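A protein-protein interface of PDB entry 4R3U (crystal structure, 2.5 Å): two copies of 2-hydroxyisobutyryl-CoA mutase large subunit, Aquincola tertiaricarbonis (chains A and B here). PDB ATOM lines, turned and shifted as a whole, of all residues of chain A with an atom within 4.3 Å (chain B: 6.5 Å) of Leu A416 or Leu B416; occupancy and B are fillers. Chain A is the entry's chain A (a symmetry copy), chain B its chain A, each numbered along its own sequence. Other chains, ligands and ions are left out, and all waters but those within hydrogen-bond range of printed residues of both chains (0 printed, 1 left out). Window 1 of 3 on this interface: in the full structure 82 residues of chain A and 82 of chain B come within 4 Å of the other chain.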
ATOM      1  N   PHE A 307      11.545  12.514   3.563  1.00  0.00           N
ATOM      2  CA  PHE A 307      11.594  11.840   4.862  1.00  0.00           C
ATOM      3  C   PHE A 307      10.440  12.118   5.775  1.00  0.00           C
ATOM      4  O   PHE A 307       9.950  11.172   6.409  1.00  0.00           O
ATOM      5  CB  PHE A 307      12.925  12.036   5.567  1.00  0.00           C
ATOM      6  CG  PHE A 307      14.052  11.340   4.849  1.00  0.00           C
ATOM      7  CD1 PHE A 307      14.137   9.950   4.838  1.00  0.00           C
ATOM      8  CD2 PHE A 307      15.006  12.068   4.154  1.00  0.00           C
ATOM      9  CE1 PHE A 307      15.176   9.307   4.173  1.00  0.00           C
ATOM     10  CE2 PHE A 307      16.036  11.420   3.487  1.00  0.00           C
ATOM     11  CZ  PHE A 307      16.120  10.042   3.514  1.00  0.00           C
ATOM     12  N   VAL A 310       7.385   9.871   4.865  1.00  0.00           N
ATOM     13  CA  VAL A 310       7.613   8.507   5.354  1.00  0.00           C
ATOM     14  C   VAL A 310       7.345   8.449   6.884  1.00  0.00           C
ATOM     15  O   VAL A 310       6.640   7.555   7.356  1.00  0.00           O
ATOM     16  CB  VAL A 310       9.044   8.011   4.995  1.00  0.00           C
ATOM     17  CG1 VAL A 310       9.316   6.638   5.593  1.00  0.00           C
ATOM     18  CG2 VAL A 310       9.263   7.994   3.478  1.00  0.00           C
ATOM     19  N   LEU A 370       8.215   3.360   0.586  1.00  0.00           N
ATOM     20  CA  LEU A 370       9.028   3.306   1.798  1.00  0.00           C
ATOM     21  C   LEU A 370       8.115   3.505   3.016  1.00  0.00           C
ATOM     22  O   LEU A 370       8.412   2.989   4.102  1.00  0.00           O
ATOM     23  CB  LEU A 370      10.157   4.367   1.748  1.00  0.00           C
ATOM     24  CG  LEU A 370      11.222   4.246   0.647  1.00  0.00           C
ATOM     25  CD1 LEU A 370      12.363   5.178   0.923  1.00  0.00           C
ATOM     26  CD2 LEU A 370      11.759   2.799   0.476  1.00  0.00           C
ATOM     27  N   ASP A 414      10.073  -2.214   5.514  1.00  0.00           N
ATOM     28  CA  ASP A 414      10.363  -0.989   6.277  1.00  0.00           C
ATOM     29  C   ASP A 414      11.894  -0.761   6.309  1.00  0.00           C
ATOM     30  O   ASP A 414      12.526  -0.866   7.376  1.00  0.00           O
ATOM     31  CB  ASP A 414       9.728  -1.042   7.687  1.00  0.00           C
ATOM     32  CG  ASP A 414       9.719   0.304   8.374  1.00  0.00           C
ATOM     33  OD1 ASP A 414       9.153   1.258   7.806  1.00  0.00           O
ATOM     34  OD2 ASP A 414      10.316   0.418   9.449  1.00  0.00           O
ATOM     35  N   PRO A 415      12.515  -0.555   5.110  1.00  0.00           N
ATOM     36  CA  PRO A 415      13.989  -0.424   5.049  1.00  0.00           C
ATOM     37  C   PRO A 415      14.535   0.755   5.836  1.00  0.00           C
ATOM     38  O   PRO A 415      15.672   0.698   6.291  1.00  0.00           O
ATOM     39  CB  PRO A 415      14.265  -0.311   3.551  1.00  0.00           C
ATOM     40  CG  PRO A 415      12.993   0.162   2.957  1.00  0.00           C
ATOM     41  CD  PRO A 415      11.923  -0.440   3.757  1.00  0.00           C
ATOM     42  N   LEU A 416      13.696   1.798   6.039  1.00  0.00           N
ATOM     43  CA  LEU A 416      14.062   2.987   6.799  1.00  0.00           C
ATOM     44  C   LEU A 416      13.943   2.775   8.309  1.00  0.00           C
ATOM     45  O   LEU A 416      14.334   3.658   9.073  1.00  0.00           O
ATOM     46  CB  LEU A 416      13.280   4.242   6.341  1.00  0.00           C
ATOM     47  CG  LEU A 416      13.387   4.685   4.871  1.00  0.00           C
ATOM     48  CD1 LEU A 416      12.950   6.134   4.708  1.00  0.00           C
ATOM     49  CD2 LEU A 416      14.775   4.550   4.350  1.00  0.00           C
ATOM     50  N   GLY A 417      13.430   1.618   8.730  1.00  0.00           N
ATOM     51  CA  GLY A 417      13.299   1.296  10.146  1.00  0.00           C
ATOM     52  C   GLY A 417      14.632   1.363  10.843  1.00  0.00           C
ATOM     53  O   GLY A 417      15.626   0.845  10.332  1.00  0.00           O
ATOM     54  N   GLY A 418      14.669   2.065  11.959  1.00  0.00           N
ATOM     55  CA  GLY A 418      15.893   2.234  12.730  1.00  0.00           C
ATOM     56  C   GLY A 418      16.626   3.529  12.483  1.00  0.00           C
ATOM     57  O   GLY A 418      17.411   3.951  13.335  1.00  0.00           O
ATOM     58  N   SER A 419      16.403   4.153  11.306  1.00  0.00           N
ATOM     59  CA  SER A 419      17.000   5.434  10.916  1.00  0.00           C
ATOM     60  C   SER A 419      16.783   6.411  12.057  1.00  0.00           C
ATOM     61  O   SER A 419      15.640   6.623  12.489  1.00  0.00           O
ATOM     62  CB  SER A 419      16.356   5.965   9.637  1.00  0.00           C
ATOM     63  OG  SER A 419      16.565   7.355   9.458  1.00  0.00           O
ATOM     64  N   VAL A 422      14.411   9.278  10.776  1.00  0.00           N
ATOM     65  CA  VAL A 422      13.050   8.826  10.484  1.00  0.00           C
ATOM     66  C   VAL A 422      12.367   8.393  11.773  1.00  0.00           C
ATOM     67  O   VAL A 422      11.227   8.793  12.015  1.00  0.00           O
ATOM     68  CB  VAL A 422      12.982   7.785   9.322  1.00  0.00           C
ATOM     69  CG1 VAL A 422      11.538   7.339   9.013  1.00  0.00           C
ATOM     70  CG2 VAL A 422      13.658   8.319   8.062  1.00  0.00           C
ATOM     71  N   ARG B  84      29.271   8.542   7.733  1.00  0.00           N
ATOM     72  CA  ARG B  84      28.181   9.513   7.558  1.00  0.00           C
ATOM     73  C   ARG B  84      28.478  10.726   6.642  1.00  0.00           C
ATOM     74  O   ARG B  84      27.580  11.515   6.368  1.00  0.00           O
ATOM     75  CB  ARG B  84      27.662   9.953   8.934  1.00  0.00           C
ATOM     76  CG  ARG B  84      27.527   8.764   9.892  1.00  0.00           C
ATOM     77  CD  ARG B  84      26.634   9.053  11.057  1.00  0.00           C
ATOM     78  NE  ARG B  84      25.257   9.172  10.620  1.00  0.00           N
ATOM     79  CZ  ARG B  84      24.316   9.798  11.302  1.00  0.00           C
ATOM     80  NH1 ARG B  84      24.598  10.360  12.471  1.00  0.00           N
ATOM     81  NH2 ARG B  84      23.079   9.876  10.821  1.00  0.00           N
ATOM     82  N   PHE B 306      18.747   0.799  -5.049  1.00  0.00           N
ATOM     83  CA  PHE B 306      18.646   1.984  -4.214  1.00  0.00           C
ATOM     84  C   PHE B 306      19.425   1.946  -2.886  1.00  0.00           C
ATOM     85  O   PHE B 306      20.284   2.802  -2.674  1.00  0.00           O
ATOM     86  CB  PHE B 306      17.168   2.372  -4.022  1.00  0.00           C
ATOM     87  CG  PHE B 306      16.972   3.703  -3.345  1.00  0.00           C
ATOM     88  CD1 PHE B 306      17.093   4.888  -4.064  1.00  0.00           C
ATOM     89  CD2 PHE B 306      16.668   3.772  -1.984  1.00  0.00           C
ATOM     90  CE1 PHE B 306      16.930   6.124  -3.440  1.00  0.00           C
ATOM     91  CE2 PHE B 306      16.476   5.007  -1.361  1.00  0.00           C
ATOM     92  CZ  PHE B 306      16.611   6.178  -2.093  1.00  0.00           C
ATOM     93  N   PHE B 307      19.129   0.958  -2.016  1.00  0.00           N
ATOM     94  CA  PHE B 307      19.772   0.827  -0.707  1.00  0.00           C
ATOM     95  C   PHE B 307      21.163   0.274  -0.726  1.00  0.00           C
ATOM     96  O   PHE B 307      22.015   0.798   0.005  1.00  0.00           O
ATOM     97  CB  PHE B 307      18.895   0.103   0.299  1.00  0.00           C
ATOM     98  CG  PHE B 307      17.675   0.907   0.667  1.00  0.00           C
ATOM     99  CD1 PHE B 307      17.790   2.063   1.434  1.00  0.00           C
ATOM    100  CD2 PHE B 307      16.418   0.532   0.218  1.00  0.00           C
ATOM    101  CE1 PHE B 307      16.665   2.808   1.772  1.00  0.00           C
ATOM    102  CE2 PHE B 307      15.300   1.283   0.552  1.00  0.00           C
ATOM    103  CZ  PHE B 307      15.431   2.410   1.340  1.00  0.00           C
ATOM    104  N   VAL B 310      23.751   3.065  -1.578  1.00  0.00           N
ATOM    105  CA  VAL B 310      23.965   3.914  -0.401  1.00  0.00           C
ATOM    106  C   VAL B 310      24.905   3.190   0.602  1.00  0.00           C
ATOM    107  O   VAL B 310      25.865   3.787   1.093  1.00  0.00           O
ATOM    108  CB  VAL B 310      22.613   4.318   0.256  1.00  0.00           C
ATOM    109  CG1 VAL B 310      22.838   5.111   1.534  1.00  0.00           C
ATOM    110  CG2 VAL B 310      21.732   5.104  -0.721  1.00  0.00           C
ATOM    111  N   ARG B 314      28.847   4.383   1.865  1.00  0.00           N
ATOM    112  CA  ARG B 314      29.163   4.511   3.293  1.00  0.00           C
ATOM    113  C   ARG B 314      30.240   3.521   3.676  1.00  0.00           C
ATOM    114  O   ARG B 314      31.193   3.896   4.374  1.00  0.00           O
ATOM    115  CB  ARG B 314      27.897   4.360   4.154  1.00  0.00           C
ATOM    116  CG  ARG B 314      26.862   5.446   3.858  1.00  0.00           C
ATOM    117  CD  ARG B 314      25.497   5.135   4.435  1.00  0.00           C
ATOM    118  NE  ARG B 314      25.354   5.636   5.803  1.00  0.00           N
ATOM    119  CZ  ARG B 314      25.463   4.891   6.897  1.00  0.00           C
ATOM    120  NH1 ARG B 314      25.721   3.589   6.803  1.00  0.00           N
ATOM    121  NH2 ARG B 314      25.310   5.441   8.097  1.00  0.00           N
ATOM    122  N   LEU B 370      21.989  10.660  -0.814  1.00  0.00           N
ATOM    123  CA  LEU B 370      21.832   9.949   0.452  1.00  0.00           C
ATOM    124  C   LEU B 370      23.162   9.266   0.803  1.00  0.00           C
ATOM    125  O   LEU B 370      23.467   9.080   1.989  1.00  0.00           O
ATOM    126  CB  LEU B 370      20.669   8.929   0.368  1.00  0.00           C
ATOM    127  CG  LEU B 370      19.248   9.465   0.130  1.00  0.00           C
ATOM    128  CD1 LEU B 370      18.239   8.379   0.353  1.00  0.00           C
ATOM    129  CD2 LEU B 370      18.901  10.689   1.018  1.00  0.00           C
ATOM    130  N   ILE B 413      21.993  15.541   7.664  1.00  0.00           N
ATOM    131  CA  ILE B 413      23.176  14.784   7.229  1.00  0.00           C
ATOM    132  C   ILE B 413      23.027  13.292   7.522  1.00  0.00           C
ATOM    133  O   ILE B 413      22.635  12.912   8.639  1.00  0.00           O
ATOM    134  CB  ILE B 413      24.529  15.376   7.735  1.00  0.00           C
ATOM    135  CG1 ILE B 413      24.633  16.867   7.393  1.00  0.00           C
ATOM    136  CG2 ILE B 413      25.730  14.615   7.126  1.00  0.00           C
ATOM    137  CD1 ILE B 413      25.515  17.590   8.217  1.00  0.00           C
ATOM    138  N   ASP B 414      23.380  12.451   6.511  1.00  0.00           N
ATOM    139  CA  ASP B 414      23.301  10.982   6.541  1.00  0.00           C
ATOM    140  C   ASP B 414      21.937  10.559   7.140  1.00  0.00           C
ATOM    141  O   ASP B 414      21.881   9.993   8.247  1.00  0.00           O
ATOM    142  CB  ASP B 414      24.508  10.368   7.289  1.00  0.00           C
ATOM    143  CG  ASP B 414      24.640   8.880   7.063  1.00  0.00           C
ATOM    144  OD1 ASP B 414      24.745   8.463   5.894  1.00  0.00           O
ATOM    145  OD2 ASP B 414      24.588   8.132   8.045  1.00  0.00           O
ATOM    146  N   PRO B 415      20.816  10.935   6.455  1.00  0.00           N
ATOM    147  CA  PRO B 415      19.475  10.650   7.013  1.00  0.00           C
ATOM    148  C   PRO B 415      19.187   9.170   7.200  1.00  0.00           C
ATOM    149  O   PRO B 415      18.402   8.817   8.074  1.00  0.00           O
ATOM    150  CB  PRO B 415      18.534  11.310   6.006  1.00  0.00           C
ATOM    151  CG  PRO B 415      19.316  11.409   4.752  1.00  0.00           C
ATOM    152  CD  PRO B 415      20.705  11.638   5.156  1.00  0.00           C
ATOM    153  N   LEU B 416      19.871   8.309   6.412  1.00  0.00           N
ATOM    154  CA  LEU B 416      19.728   6.860   6.491  1.00  0.00           C
ATOM    155  C   LEU B 416      20.548   6.254   7.631  1.00  0.00           C
ATOM    156  O   LEU B 416      20.428   5.056   7.887  1.00  0.00           O
ATOM    157  CB  LEU B 416      20.030   6.163   5.143  1.00  0.00           C
ATOM    158  CG  LEU B 416      19.204   6.555   3.905  1.00  0.00           C
ATOM    159  CD1 LEU B 416      19.312   5.491   2.822  1.00  0.00           C
ATOM    160  CD2 LEU B 416      17.766   6.749   4.235  1.00  0.00           C
ATOM    161  N   GLY B 417      21.354   7.071   8.311  1.00  0.00           N
ATOM    162  CA  GLY B 417      22.159   6.609   9.436  1.00  0.00           C
ATOM    163  C   GLY B 417      21.294   5.996  10.506  1.00  0.00           C
ATOM    164  O   GLY B 417      20.261   6.561  10.867  1.00  0.00           O
ATOM    165  N   GLY B 418      21.672   4.813  10.949  1.00  0.00           N
ATOM    166  CA  GLY B 418      20.923   4.090  11.969  1.00  0.00           C
ATOM    167  C   GLY B 418      19.984   3.036  11.440  1.00  0.00           C
ATOM    168  O   GLY B 418      19.622   2.121  12.183  1.00  0.00           O
ATOM    169  N   SER B 419      19.556   3.168  10.166  1.00  0.00           N
ATOM    170  CA  SER B 419      18.675   2.219   9.480  1.00  0.00           C
ATOM    171  C   SER B 419      19.247   0.828   9.680  1.00  0.00           C
ATOM    172  O   SER B 419      20.419   0.583   9.357  1.00  0.00           O
ATOM    173  CB  SER B 419      18.584   2.543   7.990  1.00  0.00           C
ATOM    174  OG  SER B 419      18.123   1.446   7.220  1.00  0.00           O
ATOM    175  N   TYR B 420      18.443  -0.069  10.263  1.00  0.00           N
ATOM    176  CA  TYR B 420      18.905  -1.422  10.532  1.00  0.00           C
ATOM    177  C   TYR B 420      19.439  -2.130   9.283  1.00  0.00           C
ATOM    178  O   TYR B 420      20.518  -2.709   9.326  1.00  0.00           O
ATOM    179  CB  TYR B 420      17.824  -2.229  11.247  1.00  0.00           C
ATOM    180  CG  TYR B 420      17.241  -1.567  12.477  1.00  0.00           C
ATOM    181  CD1 TYR B 420      18.066  -0.992  13.447  1.00  0.00           C
ATOM    182  CD2 TYR B 420      15.866  -1.569  12.706  1.00  0.00           C
ATOM    183  CE1 TYR B 420      17.532  -0.411  14.597  1.00  0.00           C
ATOM    184  CE2 TYR B 420      15.324  -1.028  13.870  1.00  0.00           C
ATOM    185  CZ  TYR B 420      16.159  -0.450  14.813  1.00  0.00           C
ATOM    186  OH  TYR B 420      15.586   0.112  15.927  1.00  0.00           O
ATOM    187  N   TYR B 421      18.735  -1.987   8.160  1.00  0.00           N
ATOM    188  CA  TYR B 421      19.094  -2.567   6.875  1.00  0.00           C
ATOM    189  C   TYR B 421      20.341  -1.910   6.301  1.00  0.00           C
ATOM    190  O   TYR B 421      21.305  -2.628   5.997  1.00  0.00           O
ATOM    191  CB  TYR B 421      17.888  -2.523   5.900  1.00  0.00           C
ATOM    192  CG  TYR B 421      18.185  -2.911   4.462  1.00  0.00           C
ATOM    193  CD1 TYR B 421      19.013  -3.999   4.162  1.00  0.00           C
ATOM    194  CD2 TYR B 421      17.605  -2.221   3.398  1.00  0.00           C
ATOM    195  CE1 TYR B 421      19.320  -4.337   2.846  1.00  0.00           C
ATOM    196  CE2 TYR B 421      17.883  -2.568   2.074  1.00  0.00           C
ATOM    197  CZ  TYR B 421      18.757  -3.616   1.802  1.00  0.00           C
ATOM    198  OH  TYR B 421      19.058  -3.949   0.498  1.00  0.00           O
ATOM    199  N   VAL B 422      20.347  -0.558   6.165  1.00  0.00           N
ATOM    200  CA  VAL B 422      21.474   0.166   5.576  1.00  0.00           C
ATOM    201  C   VAL B 422      22.722  -0.058   6.417  1.00  0.00           C
ATOM    202  O   VAL B 422      23.778  -0.362   5.860  1.00  0.00           O
ATOM    203  CB  VAL B 422      21.151   1.661   5.265  1.00  0.00           C
ATOM    204  CG1 VAL B 422      22.342   2.401   4.622  1.00  0.00           C
ATOM    205  CG2 VAL B 422      19.908   1.788   4.387  1.00  0.00           C
ATOM    206  N   GLU B 423      22.589  -0.033   7.751  1.00  0.00           N
ATOM    207  CA  GLU B 423      23.725  -0.283   8.646  1.00  0.00           C
ATOM    208  C   GLU B 423      24.320  -1.686   8.553  1.00  0.00           C
ATOM    209  O   GLU B 423      25.541  -1.813   8.498  1.00  0.00           O
ATOM    210  CB  GLU B 423      23.467   0.166  10.092  1.00  0.00           C
ATOM    211  CG  GLU B 423      23.268   1.670  10.271  1.00  0.00           C
ATOM    212  CD  GLU B 423      24.337   2.656   9.830  1.00  0.00           C
ATOM    213  OE1 GLU B 423      25.414   2.239   9.347  1.00  0.00           O
ATOM    214  OE2 GLU B 423      24.082   3.872   9.971  1.00  0.00           O
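Among the printed residues, pairs that only touch across the chains: Phe A307 with Leu B370, Phe A307 with Pro B415, Phe A307 with Leu B416, Leu A370 with Phe B307, Pro A415 with Phe B307, Pro A415 with Tyr B421, Leu A416 with Phe B307, Leu A416 with Leu B416, Gly A417 with Ser B419, Gly A418 with Ser B419, Gly A418 with Tyr B420, Ser A419 with Gly B417 and Ser A419 with Gly B418.
The backbone NH (N) of Ser A419 sits close to the backbone NH (N) of Ser B419 (3.5 Å). The side-chain hydroxyl (OG) of Ser B419 lies within hydrogen-bond range of the backbone carbonyl oxygen (O) of Pro A415, at 2.7 Å. The backbone carbonyl oxygen (O) of Gly A418 sits close to the backbone carbonyl oxygen (O) of Gly B418 (3.1 Å). The backbone carbonyl oxygen of Pro B415 lies within hydrogen-bond range of the side-chain hydroxyl of Ser A419. The backbone NH (N) of Tyr B420 lies within hydrogen-bond range of the backbone carbonyl oxygen (O) of Gly A417.
Of chain B, only Phe B307 (3.6 Å) and Leu B416 (3.7 Å) come within 4 Å of Leu A416. Of the printed residues of chain B, Leu A370 touches Phe B307 (3.8 Å). Of the printed residues of chain B, Phe A307 touches Leu B370 (3.8 Å), Pro B415 (3.5 Å) and Leu B416 (3.6 Å). Of the printed residues of chain A, Tyr B421 touches Pro A415. Printed residues of chain A within 4 Å of Tyr B420: Gly A417 and Gly A418. The nearest residue of chain B that does not touch Leu A416 is Ser B419 (4.4 Å). The nearest printed residue of chain A that does not touch Leu B416 is Ser A419 (4.4 Å).
Hydrophobic or aromatic side chains of chain B that line the printed part of chain A: Phe B307, Leu B370, Pro B415, Leu B416, Tyr B420 and Tyr B421. Hydrophobic or aromatic side chains of chain A within 4 Å of the printed part of chain B: Phe A307, Leu A370, Pro A415 and Leu A416. Along chain A the printed residues that touch a printed residue of chain B span positions 307 to 419.
OD2 of Asp B414 sits close to N of Gly B417 (3.4 Å). The side-chain carboxylate (OD2) of Asp A414 lies close to the backbone NH (N) of Gly A417 (3.4 Å). OG of Ser A419 is in hydrogen-bond range of N of Val A422, at 3.2 Å. The side-chain hydroxyl of Ser B419 lies within hydrogen-bond range of the backbone NH of Val B422, at 3.2 Å. The side-chain carboxylate (OE2) of Glu B423 is in hydrogen-bond range of the backbone NH (N) of Gly B418 (2.8 Å).
Phe A307 touches Leu B370, and with the chains exchanged Leu A370 touches Phe B307. Phe A307 touches Pro B415, and with the chains exchanged Pro A415 touches Phe B307. Pro A415 touches Ser B419, and with the chains exchanged Ser A419 touches Pro B415. Leu A416 touches its own counterpart, Leu B416. 10 positions are printed for both chains. Of the 18 pairs that touch across the chains among the printed residues, 15 have their exchanged pair printed and touching as well.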
